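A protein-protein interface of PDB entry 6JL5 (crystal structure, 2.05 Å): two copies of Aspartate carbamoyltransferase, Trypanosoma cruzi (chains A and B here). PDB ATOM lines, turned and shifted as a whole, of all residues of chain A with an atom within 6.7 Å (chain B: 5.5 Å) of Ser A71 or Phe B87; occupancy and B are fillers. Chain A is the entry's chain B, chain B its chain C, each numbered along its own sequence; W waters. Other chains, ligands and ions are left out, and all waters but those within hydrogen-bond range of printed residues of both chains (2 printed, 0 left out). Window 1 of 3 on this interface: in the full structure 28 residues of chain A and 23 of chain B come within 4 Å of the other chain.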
ATOM      1  N   PHE A  62       3.291 -21.636   4.779  1.00  0.00           N
ATOM      2  CA  PHE A  62       2.605 -20.506   4.221  1.00  0.00           C
ATOM      3  C   PHE A  62       1.809 -19.814   5.337  1.00  0.00           C
ATOM      4  O   PHE A  62       0.722 -20.259   5.697  1.00  0.00           O
ATOM      5  CB  PHE A  62       1.727 -20.977   3.048  1.00  0.00           C
ATOM      6  CG  PHE A  62       2.461 -20.997   1.734  1.00  0.00           C
ATOM      7  CD1 PHE A  62       3.557 -21.852   1.536  1.00  0.00           C
ATOM      8  CD2 PHE A  62       2.106 -20.117   0.707  1.00  0.00           C
ATOM      9  CE1 PHE A  62       4.265 -21.853   0.325  1.00  0.00           C
ATOM     10  CE2 PHE A  62       2.820 -20.104  -0.496  1.00  0.00           C
ATOM     11  CZ  PHE A  62       3.900 -20.975  -0.690  1.00  0.00           C
ATOM     12  N   SER A  66      -1.943 -18.478  -0.677  1.00  0.00           N
ATOM     13  CA  SER A  66      -1.431 -18.640  -2.050  1.00  0.00           C
ATOM     14  C   SER A  66      -2.187 -19.738  -2.838  1.00  0.00           C
ATOM     15  O   SER A  66      -2.709 -20.690  -2.259  1.00  0.00           O
ATOM     16  CB  SER A  66       0.074 -18.920  -2.017  1.00  0.00           C
ATOM     17  OG  SER A  66       0.534 -19.711  -3.106  1.00  0.00           O
ATOM     18  N   SER A  67      -2.271 -19.576  -4.157  1.00  0.00           N
ATOM     19  CA  SER A  67      -2.777 -20.620  -5.040  1.00  0.00           C
ATOM     20  C   SER A  67      -1.630 -21.016  -5.946  1.00  0.00           C
ATOM     21  O   SER A  67      -1.034 -22.076  -5.791  1.00  0.00           O
ATOM     22  CB  SER A  67      -3.917 -20.083  -5.909  1.00  0.00           C
ATOM     23  OG  SER A  67      -4.998 -19.628  -5.111  1.00  0.00           O
ATOM     24  N   ARG A  68      -1.312 -20.106  -6.867  1.00  0.00           N
ATOM     25  CA  ARG A  68      -0.248 -20.251  -7.826  1.00  0.00           C
ATOM     26  C   ARG A  68       0.998 -20.756  -7.155  1.00  0.00           C
ATOM     27  O   ARG A  68       1.495 -21.835  -7.496  1.00  0.00           O
ATOM     28  CB  ARG A  68       0.077 -18.889  -8.411  1.00  0.00           C
ATOM     29  CG  ARG A  68       0.044 -18.789  -9.898  1.00  0.00           C
ATOM     30  CD  ARG A  68      -0.336 -17.335 -10.232  1.00  0.00           C
ATOM     31  NE  ARG A  68      -1.290 -16.871  -9.230  1.00  0.00           N
ATOM     32  CZ  ARG A  68      -2.616 -17.018  -9.321  1.00  0.00           C
ATOM     33  NH1 ARG A  68      -3.154 -17.573 -10.399  1.00  0.00           N
ATOM     34  NH2 ARG A  68      -3.397 -16.597  -8.325  1.00  0.00           N
ATOM     35  N   THR A  69       1.490 -19.981  -6.182  1.00  0.00           N
ATOM     36  CA  THR A  69       2.819 -20.217  -5.637  1.00  0.00           C
ATOM     37  C   THR A  69       2.923 -21.562  -4.897  1.00  0.00           C
ATOM     38  O   THR A  69       3.818 -22.338  -5.197  1.00  0.00           O
ATOM     39  CB  THR A  69       3.368 -18.968  -4.849  1.00  0.00           C
ATOM     40  OG1 THR A  69       3.435 -17.845  -5.749  1.00  0.00           O
ATOM     41  CG2 THR A  69       4.731 -19.241  -4.331  1.00  0.00           C
ATOM     42  N   PHE A  70       1.990 -21.834  -3.995  1.00  0.00           N
ATOM     43  CA  PHE A  70       1.964 -23.098  -3.270  1.00  0.00           C
ATOM     44  C   PHE A  70       1.860 -24.284  -4.241  1.00  0.00           C
ATOM     45  O   PHE A  70       2.604 -25.246  -4.126  1.00  0.00           O
ATOM     46  CB  PHE A  70       0.788 -23.135  -2.292  1.00  0.00           C
ATOM     47  CG  PHE A  70       0.457 -24.528  -1.741  1.00  0.00           C
ATOM     48  CD1 PHE A  70       0.950 -24.939  -0.491  1.00  0.00           C
ATOM     49  CD2 PHE A  70      -0.401 -25.412  -2.442  1.00  0.00           C
ATOM     50  CE1 PHE A  70       0.630 -26.211   0.034  1.00  0.00           C
ATOM     51  CE2 PHE A  70      -0.729 -26.707  -1.907  1.00  0.00           C
ATOM     52  CZ  PHE A  70      -0.207 -27.091  -0.671  1.00  0.00           C
ATOM     53  N   SER A  71       0.942 -24.170  -5.198  1.00  0.00           N
ATOM     54  CA  SER A  71       0.543 -25.291  -6.023  1.00  0.00           C
ATOM     55  C   SER A  71       1.645 -25.532  -7.026  1.00  0.00           C
ATOM     56  O   SER A  71       1.976 -26.683  -7.321  1.00  0.00           O
ATOM     57  CB  SER A  71      -0.779 -24.966  -6.737  1.00  0.00           C
ATOM     58  OG  SER A  71      -1.823 -24.880  -5.801  1.00  0.00           O
ATOM     59  N   SER A  72       2.206 -24.428  -7.534  1.00  0.00           N
ATOM     60  CA  SER A  72       3.334 -24.425  -8.466  1.00  0.00           C
ATOM     61  C   SER A  72       4.521 -25.146  -7.874  1.00  0.00           C
ATOM     62  O   SER A  72       5.205 -25.956  -8.553  1.00  0.00           O
ATOM     63  CB  SER A  72       3.735 -22.954  -8.737  1.00  0.00           C
ATOM     64  OG  SER A  72       4.641 -22.834  -9.817  1.00  0.00           O
ATOM     65  N   PHE A  73       4.832 -24.797  -6.623  1.00  0.00           N
ATOM     66  CA  PHE A  73       5.943 -25.425  -5.914  1.00  0.00           C
ATOM     67  C   PHE A  73       5.701 -26.937  -5.634  1.00  0.00           C
ATOM     68  O   PHE A  73       6.603 -27.770  -5.819  1.00  0.00           O
ATOM     69  CB  PHE A  73       6.232 -24.662  -4.621  1.00  0.00           C
ATOM     70  CG  PHE A  73       7.319 -23.592  -4.753  1.00  0.00           C
ATOM     71  CD1 PHE A  73       8.635 -23.946  -4.991  1.00  0.00           C
ATOM     72  CD2 PHE A  73       7.014 -22.242  -4.612  1.00  0.00           C
ATOM     73  CE1 PHE A  73       9.616 -22.993  -5.093  1.00  0.00           C
ATOM     74  CE2 PHE A  73       8.022 -21.273  -4.667  1.00  0.00           C
ATOM     75  CZ  PHE A  73       9.304 -21.654  -4.915  1.00  0.00           C
ATOM     76  N   CYS A  74       4.504 -27.285  -5.188  1.00  0.00           N
ATOM     77  CA  CYS A  74       4.176 -28.689  -4.945  1.00  0.00           C
ATOM     78  C   CYS A  74       4.258 -29.482  -6.218  1.00  0.00           C
ATOM     79  O   CYS A  74       4.854 -30.564  -6.237  1.00  0.00           O
ATOM     80  CB  CYS A  74       2.764 -28.837  -4.358  1.00  0.00           C
ATOM     81  SG  CYS A  74       2.748 -28.316  -2.648  1.00  0.00           S
ATOM     82  N   ALA A  75       3.673 -28.935  -7.285  1.00  0.00           N
ATOM     83  CA  ALA A  75       3.694 -29.599  -8.586  1.00  0.00           C
ATOM     84  C   ALA A  75       5.106 -29.786  -9.103  1.00  0.00           C
ATOM     85  O   ALA A  75       5.439 -30.856  -9.583  1.00  0.00           O
ATOM     86  CB  ALA A  75       2.845 -28.803  -9.620  1.00  0.00           C
ATOM     87  N   ALA A  76       5.936 -28.739  -9.019  1.00  0.00           N
ATOM     88  CA  ALA A  76       7.328 -28.814  -9.428  1.00  0.00           C
ATOM     89  C   ALA A  76       8.079 -29.900  -8.680  1.00  0.00           C
ATOM     90  O   ALA A  76       8.828 -30.655  -9.295  1.00  0.00           O
ATOM     91  CB  ALA A  76       8.031 -27.450  -9.220  1.00  0.00           C
ATOM     92  N   ASN A  86       2.121 -31.945   3.610  1.00  0.00           N
ATOM     93  CA  ASN A  86       1.098 -30.892   3.522  1.00  0.00           C
ATOM     94  C   ASN A  86       0.811 -30.228   4.856  1.00  0.00           C
ATOM     95  O   ASN A  86      -0.299 -30.299   5.360  1.00  0.00           O
ATOM     96  CB  ASN A  86      -0.223 -31.420   2.916  1.00  0.00           C
ATOM     97  CG  ASN A  86      -0.208 -31.412   1.386  1.00  0.00           C
ATOM     98  OD1 ASN A  86      -0.037 -30.366   0.756  1.00  0.00           O
ATOM     99  ND2 ASN A  86      -0.382 -32.585   0.785  1.00  0.00           N
ATOM    100  N   MET A 318       6.057 -23.219 -13.353  1.00  0.00           N
ATOM    101  CA  MET A 318       6.264 -24.595 -12.866  1.00  0.00           C
ATOM    102  C   MET A 318       7.654 -25.097 -13.253  1.00  0.00           C
ATOM    103  O   MET A 318       8.352 -25.679 -12.419  1.00  0.00           O
ATOM    104  CB  MET A 318       5.187 -25.564 -13.370  1.00  0.00           C
ATOM    105  CG  MET A 318       5.378 -27.009 -12.863  1.00  0.00           C
ATOM    106  SD  MET A 318       4.089 -28.063 -13.496  1.00  0.00           S
ATOM    107  CE  MET A 318       4.679 -28.220 -15.185  1.00  0.00           C
ATOM    108  N   THR B  59      -5.435 -32.615  -9.355  1.00  0.00           N
ATOM    109  CA  THR B  59      -5.714 -31.582  -8.397  1.00  0.00           C
ATOM    110  C   THR B  59      -7.203 -31.589  -8.089  1.00  0.00           C
ATOM    111  O   THR B  59      -8.044 -31.313  -8.988  1.00  0.00           O
ATOM    112  CB  THR B  59      -5.235 -30.193  -8.874  1.00  0.00           C
ATOM    113  OG1 THR B  59      -3.869 -30.286  -9.299  1.00  0.00           O
ATOM    114  CG2 THR B  59      -5.271 -29.206  -7.745  1.00  0.00           C
ATOM    115  N   PRO B  60      -7.542 -31.912  -6.822  1.00  0.00           N
ATOM    116  CA  PRO B  60      -8.918 -31.760  -6.360  1.00  0.00           C
ATOM    117  C   PRO B  60      -9.247 -30.278  -6.265  1.00  0.00           C
ATOM    118  O   PRO B  60      -8.441 -29.515  -5.762  1.00  0.00           O
ATOM    119  CB  PRO B  60      -8.886 -32.388  -4.958  1.00  0.00           C
ATOM    120  CG  PRO B  60      -7.644 -33.258  -4.947  1.00  0.00           C
ATOM    121  CD  PRO B  60      -6.675 -32.421  -5.746  1.00  0.00           C
ATOM    122  N   LEU B  61     -10.401 -29.885  -6.791  1.00  0.00           N
ATOM    123  CA  LEU B  61     -10.922 -28.535  -6.668  1.00  0.00           C
ATOM    124  C   LEU B  61     -12.337 -28.563  -6.041  1.00  0.00           C
ATOM    125  O   LEU B  61     -13.371 -28.557  -6.731  1.00  0.00           O
ATOM    126  CB  LEU B  61     -10.892 -27.843  -8.023  1.00  0.00           C
ATOM    127  CG  LEU B  61     -11.286 -26.370  -8.062  1.00  0.00           C
ATOM    128  CD1 LEU B  61     -10.512 -25.549  -7.028  1.00  0.00           C
ATOM    129  CD2 LEU B  61     -11.055 -25.805  -9.459  1.00  0.00           C
ATOM    130  N   VAL B  85      -1.924 -32.891  -6.052  1.00  0.00           N
ATOM    131  CA  VAL B  85      -1.561 -31.577  -5.502  1.00  0.00           C
ATOM    132  C   VAL B  85      -2.743 -31.114  -4.693  1.00  0.00           C
ATOM    133  O   VAL B  85      -3.848 -31.001  -5.223  1.00  0.00           O
ATOM    134  CB  VAL B  85      -1.173 -30.545  -6.558  1.00  0.00           C
ATOM    135  CG1 VAL B  85      -1.110 -29.157  -5.913  1.00  0.00           C
ATOM    136  CG2 VAL B  85       0.184 -30.886  -7.153  1.00  0.00           C
ATOM    137  N   ASN B  86      -2.516 -30.907  -3.398  1.00  0.00           N
ATOM    138  CA  ASN B  86      -3.600 -30.619  -2.448  1.00  0.00           C
ATOM    139  C   ASN B  86      -3.984 -29.142  -2.355  1.00  0.00           C
ATOM    140  O   ASN B  86      -3.745 -28.480  -1.325  1.00  0.00           O
ATOM    141  CB  ASN B  86      -3.264 -31.193  -1.067  1.00  0.00           C
ATOM    142  CG  ASN B  86      -3.704 -32.633  -0.918  1.00  0.00           C
ATOM    143  OD1 ASN B  86      -4.901 -32.927  -0.894  1.00  0.00           O
ATOM    144  ND2 ASN B  86      -2.743 -33.544  -0.843  1.00  0.00           N
ATOM    145  N   PHE B  87      -4.563 -28.625  -3.433  1.00  0.00           N
ATOM    146  CA  PHE B  87      -5.156 -27.282  -3.459  1.00  0.00           C
ATOM    147  C   PHE B  87      -6.343 -27.067  -2.476  1.00  0.00           C
ATOM    148  O   PHE B  87      -7.332 -27.801  -2.525  1.00  0.00           O
ATOM    149  CB  PHE B  87      -5.616 -26.981  -4.892  1.00  0.00           C
ATOM    150  CG  PHE B  87      -6.173 -25.616  -5.076  1.00  0.00           C
ATOM    151  CD1 PHE B  87      -5.333 -24.552  -5.368  1.00  0.00           C
ATOM    152  CD2 PHE B  87      -7.539 -25.386  -4.953  1.00  0.00           C
ATOM    153  CE1 PHE B  87      -5.844 -23.270  -5.538  1.00  0.00           C
ATOM    154  CE2 PHE B  87      -8.063 -24.108  -5.119  1.00  0.00           C
ATOM    155  CZ  PHE B  87      -7.212 -23.046  -5.417  1.00  0.00           C
ATOM    156  N   LYS B  88      -6.256 -26.046  -1.616  1.00  0.00           N
ATOM    157  CA  LYS B  88      -7.375 -25.659  -0.725  1.00  0.00           C
ATOM    158  C   LYS B  88      -7.983 -24.304  -1.109  1.00  0.00           C
ATOM    159  O   LYS B  88      -7.261 -23.322  -1.274  1.00  0.00           O
ATOM    160  CB  LYS B  88      -6.947 -25.631   0.748  1.00  0.00           C
ATOM    161  CG  LYS B  88      -6.949 -26.998   1.430  1.00  0.00           C
ATOM    162  CD  LYS B  88      -6.925 -26.899   2.971  1.00  0.00           C
ATOM    163  CE  LYS B  88      -8.308 -27.159   3.611  1.00  0.00           C
ATOM    164  NZ  LYS B  88      -8.837 -28.558   3.410  1.00  0.00           N
ATOM    165  N   VAL B  89      -9.310 -24.267  -1.254  1.00  0.00           N
ATOM    166  CA  VAL B  89     -10.056 -23.032  -1.569  1.00  0.00           C
ATOM    167  C   VAL B  89     -10.021 -22.009  -0.410  1.00  0.00           C
ATOM    168  O   VAL B  89      -9.902 -20.793  -0.652  1.00  0.00           O
ATOM    169  CB  VAL B  89     -11.506 -23.365  -2.045  1.00  0.00           C
ATOM    170  CG1 VAL B  89     -12.454 -22.185  -1.899  1.00  0.00           C
ATOM    171  CG2 VAL B  89     -11.481 -23.882  -3.492  1.00  0.00           C
ATOM    172  N   SER B  92      -6.512 -20.050  -0.277  1.00  0.00           N
ATOM    173  CA  SER B  92      -6.099 -19.671  -1.637  1.00  0.00           C
ATOM    174  C   SER B  92      -6.247 -18.180  -1.988  1.00  0.00           C
ATOM    175  O   SER B  92      -6.737 -17.370  -1.187  1.00  0.00           O
ATOM    176  CB  SER B  92      -6.861 -20.528  -2.673  1.00  0.00           C
ATOM    177  OG  SER B  92      -8.214 -20.125  -2.806  1.00  0.00           O
ATOM    178  N   ILE B  94      -8.373 -16.906  -4.076  1.00  0.00           N
ATOM    179  CA  ILE B  94      -9.790 -16.484  -4.109  1.00  0.00           C
ATOM    180  C   ILE B  94     -10.032 -15.357  -3.078  1.00  0.00           C
ATOM    181  O   ILE B  94     -10.716 -14.358  -3.360  1.00  0.00           O
ATOM    182  CB  ILE B  94     -10.763 -17.687  -3.874  1.00  0.00           C
ATOM    183  CG1 ILE B  94     -10.797 -18.581  -5.118  1.00  0.00           C
ATOM    184  CG2 ILE B  94     -12.189 -17.209  -3.498  1.00  0.00           C
ATOM    185  CD1 ILE B  94     -11.246 -20.013  -4.862  1.00  0.00           C
ATOM    186  N   THR B 103      -8.996 -19.322 -11.386  1.00  0.00           N
ATOM    187  CA  THR B 103      -8.659 -20.486 -10.542  1.00  0.00           C
ATOM    188  C   THR B 103      -8.482 -21.777 -11.381  1.00  0.00           C
ATOM    189  O   THR B 103      -7.447 -22.462 -11.264  1.00  0.00           O
ATOM    190  CB  THR B 103      -9.697 -20.645  -9.410  1.00  0.00           C
ATOM    191  OG1 THR B 103      -9.631 -19.490  -8.567  1.00  0.00           O
ATOM    192  CG2 THR B 103      -9.432 -21.897  -8.540  1.00  0.00           C
ATOM    193  N   LEU B 107      -4.908 -24.085 -11.783  1.00  0.00           N
ATOM    194  CA  LEU B 107      -4.663 -25.533 -11.568  1.00  0.00           C
ATOM    195  C   LEU B 107      -4.345 -26.245 -12.875  1.00  0.00           C
ATOM    196  O   LEU B 107      -3.559 -27.193 -12.931  1.00  0.00           O
ATOM    197  CB  LEU B 107      -5.869 -26.211 -10.894  1.00  0.00           C
ATOM    198  CG  LEU B 107      -5.945 -26.007  -9.377  1.00  0.00           C
ATOM    199  CD1 LEU B 107      -5.712 -24.585  -8.943  1.00  0.00           C
ATOM    200  CD2 LEU B 107      -7.318 -26.509  -8.895  1.00  0.00           C
ATOM    201  N   TYR B 110      -0.555 -26.832 -14.198  1.00  0.00           N
ATOM    202  CA  TYR B 110       0.332 -27.760 -13.490  1.00  0.00           C
ATOM    203  C   TYR B 110      -0.168 -29.204 -13.484  1.00  0.00           C
ATOM    204  O   TYR B 110       0.594 -30.113 -13.186  1.00  0.00           O
ATOM    205  CB  TYR B 110       0.478 -27.339 -12.017  1.00  0.00           C
ATOM    206  CG  TYR B 110       0.601 -25.854 -11.761  1.00  0.00           C
ATOM    207  CD1 TYR B 110       1.620 -25.108 -12.346  1.00  0.00           C
ATOM    208  CD2 TYR B 110      -0.279 -25.209 -10.898  1.00  0.00           C
ATOM    209  CE1 TYR B 110       1.754 -23.766 -12.096  1.00  0.00           C
ATOM    210  CE2 TYR B 110      -0.153 -23.851 -10.638  1.00  0.00           C
ATOM    211  CZ  TYR B 110       0.863 -23.147 -11.248  1.00  0.00           C
ATOM    212  OH  TYR B 110       0.969 -21.823 -11.009  1.00  0.00           O
HETATM  213  O   HOH W   1       3.434 -21.142 -11.495  1.00  0.00           O
HETATM  214  O   HOH W   2       0.239 -30.595  -2.063  1.00  0.00           O
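ND2 of Asn A86 lies close to ND2 of Asn B86, 3.0 Å away.
OG of Ser A66 is in hydrogen-bond range of N of Thr A69 (3.2 Å). The backbone NH of Ile B94 lies close to the side-chain hydroxyl of Ser B92 (3.5 Å). The side-chain hydroxyl (OG) of Ser A66 is in hydrogen-bond range of the backbone NH (N) of Phe A70, 2.7 Å away. The side-chain hydroxyl of Ser B92 lies within hydrogen-bond range of the backbone carbonyl oxygen of Val B89, 2.8 Å away. OG of Ser A71 is in hydrogen-bond range of O of Ser A67, 2.9 Å away. The side-chain sulfur (SG) of Cys A74 sits at hydrogen-bond distance from the backbone carbonyl oxygen (O) of Phe A70 (3.4 Å).
Among the printed residues, merely in contact across the chains: Ser A67 with Ser B92 (3.2 Å), Arg A68 with Tyr B110 (3.4 Å), Phe A70 with Asn B86 (3.5 Å), Ser A71 with Phe B87 (3.6 Å), Ser A66 with Ser B92 (3.6 Å), Ala A75 with Tyr B110 (3.7 Å), Met A318 with Tyr B110 (3.7 Å), Ser A67 with Phe B87 (3.7 Å), Ser A72 with Tyr B110 (3.8 Å) and Ala A75 with Val B85 (3.9996 Å).
Of the printed residues of chain B, Ser A67 touches Phe B87 (3.7 Å) and Ser B92 (3.2 Å). Thr A69 touches none of the printed residues of chain B. Printed residues of chain B within 4 Å of Ser A71: Phe B87 (3.6 Å). Printed residues of chain B within 4 Å of Asn A86: Asn B86 (3.0 Å). Printed residues of chain B within 4 Å of Met A318: Tyr B110. Of the printed residues of chain A, Asn B86 touches Phe A70 and Asn A86. Of chain A, only Ser A67 (3.7 Å) and Ser A71 (3.6 Å) come within 4 Å of Phe B87. Lys B88 touches none of the printed residues of chain A. Of the printed residues of chain A, Ser B92 touches Ser A66 and Ser A67. The nearest printed residue of chain B that does not touch Ser A71 is Tyr B110 (4.1 Å). The nearest residue of chain A that does not touch Phe B87 is Phe A70 (4.6 Å). The nearest printed residue of chain B that does not touch Ser A72 is Val B85 (6.0 Å).
Hydrophobic or aromatic side chains of chain B that line the printed part of chain A: Val B85, Phe B87 and Tyr B110. Printed residues of chain A that touch a printed residue of chain B: Ser A66, Ser A67, Arg A68, Phe A70, Ser A71, Ser A72, Ala A75, Asn A86 and Met A318. Hydrophobic or aromatic side chains of chain A that line the printed part of chain B: Phe A70, Ala A75 and Met A318. Among the printed residues, 11 pairs touch across the chains.
Asn A86 touches its own counterpart, Asn B86. Of the 11 pairs that touch across the chains among the printed residues, 1 has its exchanged pair printed and touching as well.
Water W1 bridges OH of Tyr B110 and OG of Ser A72. Water W2 lies within hydrogen-bond range of OD1 of Asn A86 (2.8 Å), N of Asn B86 (3.1 Å) and SG of Cys A74 (3.4 Å).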
